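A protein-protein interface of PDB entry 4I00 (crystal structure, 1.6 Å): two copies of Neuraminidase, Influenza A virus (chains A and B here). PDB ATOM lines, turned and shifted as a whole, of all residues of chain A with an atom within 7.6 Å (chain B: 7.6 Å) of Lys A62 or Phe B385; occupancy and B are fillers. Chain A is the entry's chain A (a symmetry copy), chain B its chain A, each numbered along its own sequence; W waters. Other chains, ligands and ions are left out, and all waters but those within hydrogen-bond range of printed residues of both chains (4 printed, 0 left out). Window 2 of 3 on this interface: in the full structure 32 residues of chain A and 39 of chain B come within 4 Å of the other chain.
Printed residues of chain B within 4 Å of Lys A31: Asn B30. Lys A62 touches just these residues of chain B: Glu B29 (2.9 Å) and Phe B385 (3.4 Å). Of the printed residues of chain A, Asn B30 touches Lys A31 (3.9 Å). Of the printed residues of chain A, Ser B381 touches His A63. No residue of chain A comes within 4 Å of Gly B384. Of chain A, only Lys A62 (3.4 Å) and His A63 (3.8 Å) come within 4 Å of Phe B385. Of the printed residues of chain A, Met B386 touches His A63. Lys B388 touches none of the printed residues of chain A. The nearest residue of chain B that does not touch Lys A62 is Gly B384 (5.3 Å).
Hydrophobic or aromatic side chains of chain A within 4 Å of the printed part of chain B: His A63. Of the 13 printed residues of chain B, 7 touch a printed residue of chain A. Among the printed residues, 10 pairs touch across the chains. Among the printed residues, no Asp or Glu carboxylate lies within 4 Å of a Lys or Arg side-chain nitrogen of the other chain.
The backbone carbonyl oxygen (O) of Gly B380 sits at hydrogen-bond distance from the guanidinium group (NH2) of Arg B26 (3.1 Å). The side-chain amide oxygen of Asn B382 lies close to the backbone NH of Gly B384 (3.0 Å). N of Arg B26 is in hydrogen-bond range of OG of Ser B381, 3.0 Å away. O of Thr A61 sits at hydrogen-bond distance from OG of Ser A64. The backbone carbonyl oxygen of Leu A58 lies within hydrogen-bond range of the side-chain hydroxyl of Thr A61 (2.6 Å).
Water W4 lies within hydrogen-bond range of the backbone carbonyl oxygen (O) of Phe B385 (2.7 Å), the side-chain carboxylate (OE2) of Glu B29 (2.7 Å) and the side-chain amino group (NZ) of Lys A62 (2.9 Å). Water W1 bridges OD1 of Asn B30 (2.7 Å) and O of Lys A31 (2.8 Å). Water W2 lies within hydrogen-bond range of OG1 of Thr A61 (2.7 Å), N of Leu A58 (2.8 Å) and O of Arg B26 (2.8 Å). Water W3 bridges NH1 of Arg B26 (2.9 Å) and O of His A63 (3.0 Å).
The side-chain carboxylate (OE2) of Glu B29 sits at hydrogen-bond distance from the backbone NH (N) of Lys A62, 2.9 Å away. The side-chain hydroxyl (OG1) of Thr A61 sits close to the side-chain carboxylate (OE1) of Glu B29, at 3.4 Å. OE1 of Glu B29 is in hydrogen-bond range of ND1 of His A63, at 2.8 Å. NE2 of His A63 lies within hydrogen-bond range of N of Asn B382 (2.9 Å).
Position printed for both chains: 388.
OD1 of Asn B30 touches CB of Lys A31 (3.9 Å). CD of Lys A62 touches CD1 of Phe B385, 3.4 Å away. CD2 of His A63 touches NH2 of Arg B26, 3.9 Å away. Ser B381 touches His A63. His A63 touches Phe B385. His A63 touches Met B386.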
ATOM      1  N   LYS A  31     -38.489  -0.588  12.045  1.00  0.00           N
ATOM      2  CA  LYS A  31     -37.458  -1.535  11.615  1.00  0.00           C
ATOM      3  C   LYS A  31     -37.865  -2.416  10.436  1.00  0.00           C
ATOM      4  O   LYS A  31     -37.416  -3.555  10.338  1.00  0.00           O
ATOM      5  CB  LYS A  31     -37.003  -2.417  12.786  1.00  0.00           C
ATOM      6  CG  LYS A  31     -36.339  -1.645  13.918  1.00  0.00           C
ATOM      7  CD  LYS A  31     -36.097  -2.537  15.121  1.00  0.00           C
ATOM      8  CE  LYS A  31     -35.625  -1.739  16.332  1.00  0.00           C
ATOM      9  NZ  LYS A  31     -35.245  -2.649  17.453  1.00  0.00           N
ATOM     10  N   ALA A  57     -28.735  -5.172   6.107  1.00  0.00           N
ATOM     11  CA  ALA A  57     -29.278  -5.018   7.449  1.00  0.00           C
ATOM     12  C   ALA A  57     -30.557  -4.191   7.411  1.00  0.00           C
ATOM     13  O   ALA A  57     -30.752  -3.380   6.505  1.00  0.00           O
ATOM     14  CB  ALA A  57     -28.241  -4.345   8.366  1.00  0.00           C
ATOM     15  N   LEU A  58     -31.415  -4.395   8.402  1.00  0.00           N
ATOM     16  CA  LEU A  58     -32.624  -3.587   8.545  1.00  0.00           C
ATOM     17  C   LEU A  58     -32.340  -2.361   9.408  1.00  0.00           C
ATOM     18  O   LEU A  58     -31.653  -2.459  10.428  1.00  0.00           O
ATOM     19  CB  LEU A  58     -33.756  -4.406   9.164  1.00  0.00           C
ATOM     20  CG  LEU A  58     -34.297  -5.550   8.311  1.00  0.00           C
ATOM     21  CD1 LEU A  58     -35.429  -6.261   9.038  1.00  0.00           C
ATOM     22  CD2 LEU A  58     -34.782  -5.015   6.961  1.00  0.00           C
ATOM     23  N   LEU A  59     -32.889  -1.222   9.000  1.00  0.00           N
ATOM     24  CA  LEU A  59     -32.695   0.048   9.696  1.00  0.00           C
ATOM     25  C   LEU A  59     -33.155  -0.075  11.146  1.00  0.00           C
ATOM     26  O   LEU A  59     -34.272  -0.504  11.420  1.00  0.00           O
ATOM     27  CB  LEU A  59     -33.472   1.148   8.967  1.00  0.00           C
ATOM     28  CG  LEU A  59     -33.341   2.637   9.311  1.00  0.00           C
ATOM     29  CD1 LEU A  59     -33.907   2.949  10.690  1.00  0.00           C
ATOM     30  CD2 LEU A  59     -31.918   3.113   9.175  1.00  0.00           C
ATOM     31  N   GLY A  60     -32.271   0.277  12.079  1.00  0.00           N
ATOM     32  CA  GLY A  60     -32.608   0.274  13.491  1.00  0.00           C
ATOM     33  C   GLY A  60     -32.326  -1.020  14.229  1.00  0.00           C
ATOM     34  O   GLY A  60     -32.576  -1.109  15.433  1.00  0.00           O
ATOM     35  N   THR A  61     -31.827  -2.030  13.515  1.00  0.00           N
ATOM     36  CA  THR A  61     -31.397  -3.276  14.148  1.00  0.00           C
ATOM     37  C   THR A  61     -29.928  -3.156  14.515  1.00  0.00           C
ATOM     38  O   THR A  61     -29.252  -2.220  14.085  1.00  0.00           O
ATOM     39  CB  THR A  61     -31.591  -4.516  13.231  1.00  0.00           C
ATOM     40  OG1 THR A  61     -30.808  -4.371  12.038  1.00  0.00           O
ATOM     41  CG2 THR A  61     -33.058  -4.694  12.862  1.00  0.00           C
ATOM     42  N   LYS A  62     -29.427  -4.102  15.301  1.00  0.00           N
ATOM     43  CA  LYS A  62     -28.029  -4.050  15.731  1.00  0.00           C
ATOM     44  C   LYS A  62     -27.061  -4.114  14.550  1.00  0.00           C
ATOM     45  O   LYS A  62     -25.987  -3.503  14.578  1.00  0.00           O
ATOM     46  CB  LYS A  62     -27.726  -5.159  16.740  1.00  0.00           C
ATOM     47  CG  LYS A  62     -28.492  -5.030  18.048  1.00  0.00           C
ATOM     48  CD  LYS A  62     -28.224  -6.219  18.954  1.00  0.00           C
ATOM     49  CE  LYS A  62     -28.877  -6.051  20.317  1.00  0.00           C
ATOM     50  NZ  LYS A  62     -30.357  -6.025  20.231  1.00  0.00           N
ATOM     51  N   HIS A  63     -27.435  -4.849  13.508  1.00  0.00           N
ATOM     52  CA  HIS A  63     -26.588  -4.946  12.322  1.00  0.00           C
ATOM     53  C   HIS A  63     -26.506  -3.638  11.530  1.00  0.00           C
ATOM     54  O   HIS A  63     -25.650  -3.503  10.666  1.00  0.00           O
ATOM     55  CB  HIS A  63     -27.042  -6.088  11.410  1.00  0.00           C
ATOM     56  CG  HIS A  63     -26.628  -7.448  11.891  1.00  0.00           C
ATOM     57  ND1 HIS A  63     -27.461  -8.258  12.625  1.00  0.00           N
ATOM     58  CD2 HIS A  63     -25.466  -8.126  11.746  1.00  0.00           C
ATOM     59  CE1 HIS A  63     -26.830  -9.387  12.915  1.00  0.00           C
ATOM     60  NE2 HIS A  63     -25.620  -9.332  12.386  1.00  0.00           N
ATOM     61  N   SER A  64     -27.387  -2.680  11.817  1.00  0.00           N
ATOM     62  CA  SER A  64     -27.338  -1.397  11.107  1.00  0.00           C
ATOM     63  C   SER A  64     -26.305  -0.455  11.730  1.00  0.00           C
ATOM     64  O   SER A  64     -25.882   0.524  11.105  1.00  0.00           O
ATOM     65  CB  SER A  64     -28.710  -0.725  11.053  1.00  0.00           C
ATOM     66  OG  SER A  64     -29.132  -0.282  12.330  1.00  0.00           O
ATOM     67  N   ASN A  65     -25.893  -0.776  12.955  1.00  0.00           N
ATOM     68  CA  ASN A  65     -24.869  -0.008  13.666  1.00  0.00           C
ATOM     69  C   ASN A  65     -23.561   0.001  12.880  1.00  0.00           C
ATOM     70  O   ASN A  65     -22.981  -1.047  12.621  1.00  0.00           O
ATOM     71  CB  ASN A  65     -24.653  -0.616  15.058  1.00  0.00           C
ATOM     72  CG  ASN A  65     -23.754   0.230  15.955  1.00  0.00           C
ATOM     73  OD1 ASN A  65     -22.825   0.889  15.487  1.00  0.00           O
ATOM     74  ND2 ASN A  65     -24.033   0.196  17.263  1.00  0.00           N
ATOM     75  N   GLY A  66     -23.109   1.186  12.482  1.00  0.00           N
ATOM     76  CA  GLY A  66     -21.829   1.313  11.810  1.00  0.00           C
ATOM     77  C   GLY A  66     -21.891   1.276  10.294  1.00  0.00           C
ATOM     78  O   GLY A  66     -20.858   1.162   9.613  1.00  0.00           O
ATOM     79  N   THR A  67     -23.103   1.381   9.754  1.00  0.00           N
ATOM     80  CA  THR A  67     -23.279   1.350   8.309  1.00  0.00           C
ATOM     81  C   THR A  67     -22.821   2.618   7.588  1.00  0.00           C
ATOM     82  O   THR A  67     -23.031   2.751   6.386  1.00  0.00           O
ATOM     83  CB  THR A  67     -24.736   1.018   7.916  1.00  0.00           C
ATOM     84  OG1 THR A  67     -25.628   1.741   8.768  1.00  0.00           O
ATOM     85  CG2 THR A  67     -24.996  -0.478   8.064  1.00  0.00           C
ATOM     86  N   SER A 356     -26.790   5.194  15.390  1.00  0.00           N
ATOM     87  CA  SER A 356     -25.572   4.452  15.069  1.00  0.00           C
ATOM     88  C   SER A 356     -25.473   4.098  13.585  1.00  0.00           C
ATOM     89  O   SER A 356     -24.395   3.756  13.094  1.00  0.00           O
ATOM     90  CB  SER A 356     -25.445   3.186  15.930  1.00  0.00           C
ATOM     91  OG  SER A 356     -26.303   2.142  15.489  1.00  0.00           O
ATOM     92  N   LYS A 388     -32.028   3.672  17.392  1.00  0.00           N
ATOM     93  CA  LYS A 388     -30.673   4.133  17.131  1.00  0.00           C
ATOM     94  C   LYS A 388     -29.756   3.035  16.595  1.00  0.00           C
ATOM     95  O   LYS A 388     -30.011   1.833  16.739  1.00  0.00           O
ATOM     96  CB  LYS A 388     -30.072   4.766  18.390  1.00  0.00           C
ATOM     97  CG  LYS A 388     -30.871   5.948  18.929  1.00  0.00           C
ATOM     98  CD  LYS A 388     -30.153   6.615  20.101  1.00  0.00           C
ATOM     99  CE  LYS A 388     -30.980   7.744  20.696  1.00  0.00           C
ATOM    100  NZ  LYS A 388     -31.245   8.840  19.722  1.00  0.00           N
ATOM    101  OXT LYS A 388     -28.725   3.336  15.997  1.00  0.00           O
ATOM    102  N   ARG B  26     -28.412 -11.909   8.687  1.00  0.00           N
ATOM    103  CA  ARG B  26     -28.325 -10.510   9.091  1.00  0.00           C
ATOM    104  C   ARG B  26     -29.704  -9.836   9.005  1.00  0.00           C
ATOM    105  O   ARG B  26     -30.154  -9.180   9.945  1.00  0.00           O
ATOM    106  CB  ARG B  26     -27.318  -9.761   8.210  1.00  0.00           C
ATOM    107  CG  ARG B  26     -25.857 -10.158   8.424  1.00  0.00           C
ATOM    108  CD  ARG B  26     -24.970  -9.596   7.326  1.00  0.00           C
ATOM    109  NE  ARG B  26     -25.108  -8.145   7.172  1.00  0.00           N
ATOM    110  CZ  ARG B  26     -24.315  -7.238   7.746  1.00  0.00           C
ATOM    111  NH1 ARG B  26     -24.523  -5.948   7.535  1.00  0.00           N
ATOM    112  NH2 ARG B  26     -23.311  -7.618   8.527  1.00  0.00           N
ATOM    113  N   GLU B  29     -32.646 -10.518  11.767  1.00  0.00           N
ATOM    114  CA  GLU B  29     -32.466 -10.134  13.163  1.00  0.00           C
ATOM    115  C   GLU B  29     -33.789  -9.774  13.843  1.00  0.00           C
ATOM    116  O   GLU B  29     -33.975 -10.037  15.036  1.00  0.00           O
ATOM    117  CB  GLU B  29     -31.464  -8.973  13.272  1.00  0.00           C
ATOM    118  CG  GLU B  29     -30.966  -8.713  14.684  1.00  0.00           C
ATOM    119  CD  GLU B  29     -30.314  -7.353  14.825  1.00  0.00           C
ATOM    120  OE1 GLU B  29     -29.554  -6.960  13.920  1.00  0.00           O
ATOM    121  OE2 GLU B  29     -30.587  -6.661  15.828  1.00  0.00           O
ATOM    122  N   ASN B  30     -34.721  -9.195  13.087  1.00  0.00           N
ATOM    123  CA  ASN B  30     -36.007  -8.793  13.661  1.00  0.00           C
ATOM    124  C   ASN B  30     -37.138  -9.812  13.408  1.00  0.00           C
ATOM    125  O   ASN B  30     -38.316  -9.456  13.417  1.00  0.00           O
ATOM    126  CB  ASN B  30     -36.394  -7.396  13.155  1.00  0.00           C
ATOM    127  CG  ASN B  30     -37.338  -6.668  14.097  1.00  0.00           C
ATOM    128  OD1 ASN B  30     -38.282  -6.010  13.656  1.00  0.00           O
ATOM    129  ND2 ASN B  30     -37.094  -6.788  15.398  1.00  0.00           N
ATOM    130  N   VAL B 355     -27.245 -20.043  19.646  1.00  0.00           N
ATOM    131  CA  VAL B 355     -28.674 -19.877  19.418  1.00  0.00           C
ATOM    132  C   VAL B 355     -29.332 -21.254  19.397  1.00  0.00           C
ATOM    133  O   VAL B 355     -28.638 -22.273  19.310  1.00  0.00           O
ATOM    134  CB  VAL B 355     -28.955 -19.143  18.091  1.00  0.00           C
ATOM    135  CG1 VAL B 355     -28.414 -17.727  18.143  1.00  0.00           C
ATOM    136  CG2 VAL B 355     -28.351 -19.899  16.922  1.00  0.00           C
ATOM    137  N   GLY B 380     -21.739 -13.156   7.505  1.00  0.00           N
ATOM    138  CA  GLY B 380     -21.622 -11.796   7.989  1.00  0.00           C
ATOM    139  C   GLY B 380     -22.440 -11.451   9.218  1.00  0.00           C
ATOM    140  O   GLY B 380     -22.378 -10.317   9.694  1.00  0.00           O
ATOM    141  N   SER B 381     -23.208 -12.409   9.730  1.00  0.00           N
ATOM    142  CA  SER B 381     -24.015 -12.182  10.926  1.00  0.00           C
ATOM    143  C   SER B 381     -23.185 -12.181  12.202  1.00  0.00           C
ATOM    144  O   SER B 381     -22.321 -13.032  12.390  1.00  0.00           O
ATOM    145  CB  SER B 381     -25.110 -13.241  11.062  1.00  0.00           C
ATOM    146  OG  SER B 381     -26.029 -13.128   9.998  1.00  0.00           O
ATOM    147  N   ASN B 382     -23.460 -11.216  13.072  1.00  0.00           N
ATOM    148  CA  ASN B 382     -22.943 -11.244  14.429  1.00  0.00           C
ATOM    149  C   ASN B 382     -23.925 -12.061  15.248  1.00  0.00           C
ATOM    150  O   ASN B 382     -24.991 -11.570  15.620  1.00  0.00           O
ATOM    151  CB  ASN B 382     -22.824  -9.820  14.975  1.00  0.00           C
ATOM    152  CG  ASN B 382     -22.214  -9.767  16.363  1.00  0.00           C
ATOM    153  OD1 ASN B 382     -22.423 -10.662  17.182  1.00  0.00           O
ATOM    154  ND2 ASN B 382     -21.467  -8.699  16.640  1.00  0.00           N
ATOM    155  N   ILE B 383     -23.582 -13.321  15.508  1.00  0.00           N
ATOM    156  CA  ILE B 383     -24.537 -14.243  16.111  1.00  0.00           C
ATOM    157  C   ILE B 383     -25.035 -13.719  17.456  1.00  0.00           C
ATOM    158  O   ILE B 383     -26.121 -14.083  17.919  1.00  0.00           O
ATOM    159  CB  ILE B 383     -23.947 -15.647  16.275  1.00  0.00           C
ATOM    160  CG1 ILE B 383     -25.070 -16.679  16.396  1.00  0.00           C
ATOM    161  CG2 ILE B 383     -22.998 -15.687  17.462  1.00  0.00           C
ATOM    162  CD1 ILE B 383     -25.933 -16.785  15.143  1.00  0.00           C
ATOM    163  N   GLY B 384     -24.243 -12.842  18.069  1.00  0.00           N
ATOM    164  CA  GLY B 384     -24.608 -12.253  19.343  1.00  0.00           C
ATOM    165  C   GLY B 384     -25.757 -11.267  19.254  1.00  0.00           C
ATOM    166  O   GLY B 384     -26.416 -10.995  20.253  1.00  0.00           O
ATOM    167  N   PHE B 385     -25.992 -10.722  18.065  1.00  0.00           N
ATOM    168  CA  PHE B 385     -27.081  -9.764  17.875  1.00  0.00           C
ATOM    169  C   PHE B 385     -28.422 -10.467  17.689  1.00  0.00           C
ATOM    170  O   PHE B 385     -29.477  -9.840  17.782  1.00  0.00           O
ATOM    171  CB  PHE B 385     -26.827  -8.885  16.643  1.00  0.00           C
ATOM    172  CG  PHE B 385     -25.706  -7.897  16.803  1.00  0.00           C
ATOM    173  CD1 PHE B 385     -25.231  -7.545  18.057  1.00  0.00           C
ATOM    174  CD2 PHE B 385     -25.140  -7.300  15.686  1.00  0.00           C
ATOM    175  CE1 PHE B 385     -24.193  -6.624  18.192  1.00  0.00           C
ATOM    176  CE2 PHE B 385     -24.102  -6.377  15.810  1.00  0.00           C
ATOM    177  CZ  PHE B 385     -23.632  -6.040  17.066  1.00  0.00           C
ATOM    178  N   MET B 386     -28.376 -11.768  17.421  1.00  0.00           N
ATOM    179  CA  MET B 386     -29.564 -12.502  17.002  1.00  0.00           C
ATOM    180  C   MET B 386     -30.457 -12.974  18.147  1.00  0.00           C
ATOM    181  O   MET B 386     -29.973 -13.321  19.224  1.00  0.00           O
ATOM    182  CB  MET B 386     -29.169 -13.711  16.151  1.00  0.00           C
ATOM    183  CG  MET B 386     -28.334 -13.388  14.936  1.00  0.00           C
ATOM    184  SD  MET B 386     -29.194 -12.374  13.722  1.00  0.00           S
ATOM    185  CE  MET B 386     -30.564 -13.445  13.275  1.00  0.00           C
ATOM    186  N   PRO B 387     -31.777 -12.993  17.904  1.00  0.00           N
ATOM    187  CA  PRO B 387     -32.734 -13.664  18.785  1.00  0.00           C
ATOM    188  C   PRO B 387     -32.402 -15.153  18.807  1.00  0.00           C
ATOM    189  O   PRO B 387     -32.266 -15.763  17.746  1.00  0.00           O
ATOM    190  CB  PRO B 387     -34.077 -13.440  18.080  1.00  0.00           C
ATOM    191  CG  PRO B 387     -33.722 -13.078  16.662  1.00  0.00           C
ATOM    192  CD  PRO B 387     -32.440 -12.330  16.770  1.00  0.00           C
ATOM    193  N   LYS B 388     -32.269 -15.731  19.995  1.00  0.00           N
ATOM    194  CA  LYS B 388     -31.782 -17.098  20.107  1.00  0.00           C
ATOM    195  C   LYS B 388     -32.869 -18.145  19.868  1.00  0.00           C
ATOM    196  O   LYS B 388     -34.073 -17.881  19.962  1.00  0.00           O
ATOM    197  CB  LYS B 388     -31.117 -17.317  21.469  1.00  0.00           C
ATOM    198  CG  LYS B 388     -29.944 -16.381  21.742  1.00  0.00           C
ATOM    199  CD  LYS B 388     -29.243 -16.737  23.052  1.00  0.00           C
ATOM    200  CE  LYS B 388     -28.123 -15.760  23.372  1.00  0.00           C
ATOM    201  NZ  LYS B 388     -27.048 -15.755  22.340  1.00  0.00           N
ATOM    202  OXT LYS B 388     -32.554 -19.296  19.570  1.00  0.00           O
HETATM  203  O   HOH W   1     -38.866  -5.874  11.016  1.00  0.00           O
HETATM  204  O   HOH W   2     -30.752  -6.423  10.267  1.00  0.00           O
HETATM  205  O   HOH W   3     -23.001  -4.154   9.313  1.00  0.00           O
HETATM  206  O   HOH W   4     -31.224  -7.848  18.183  1.00  0.00           O
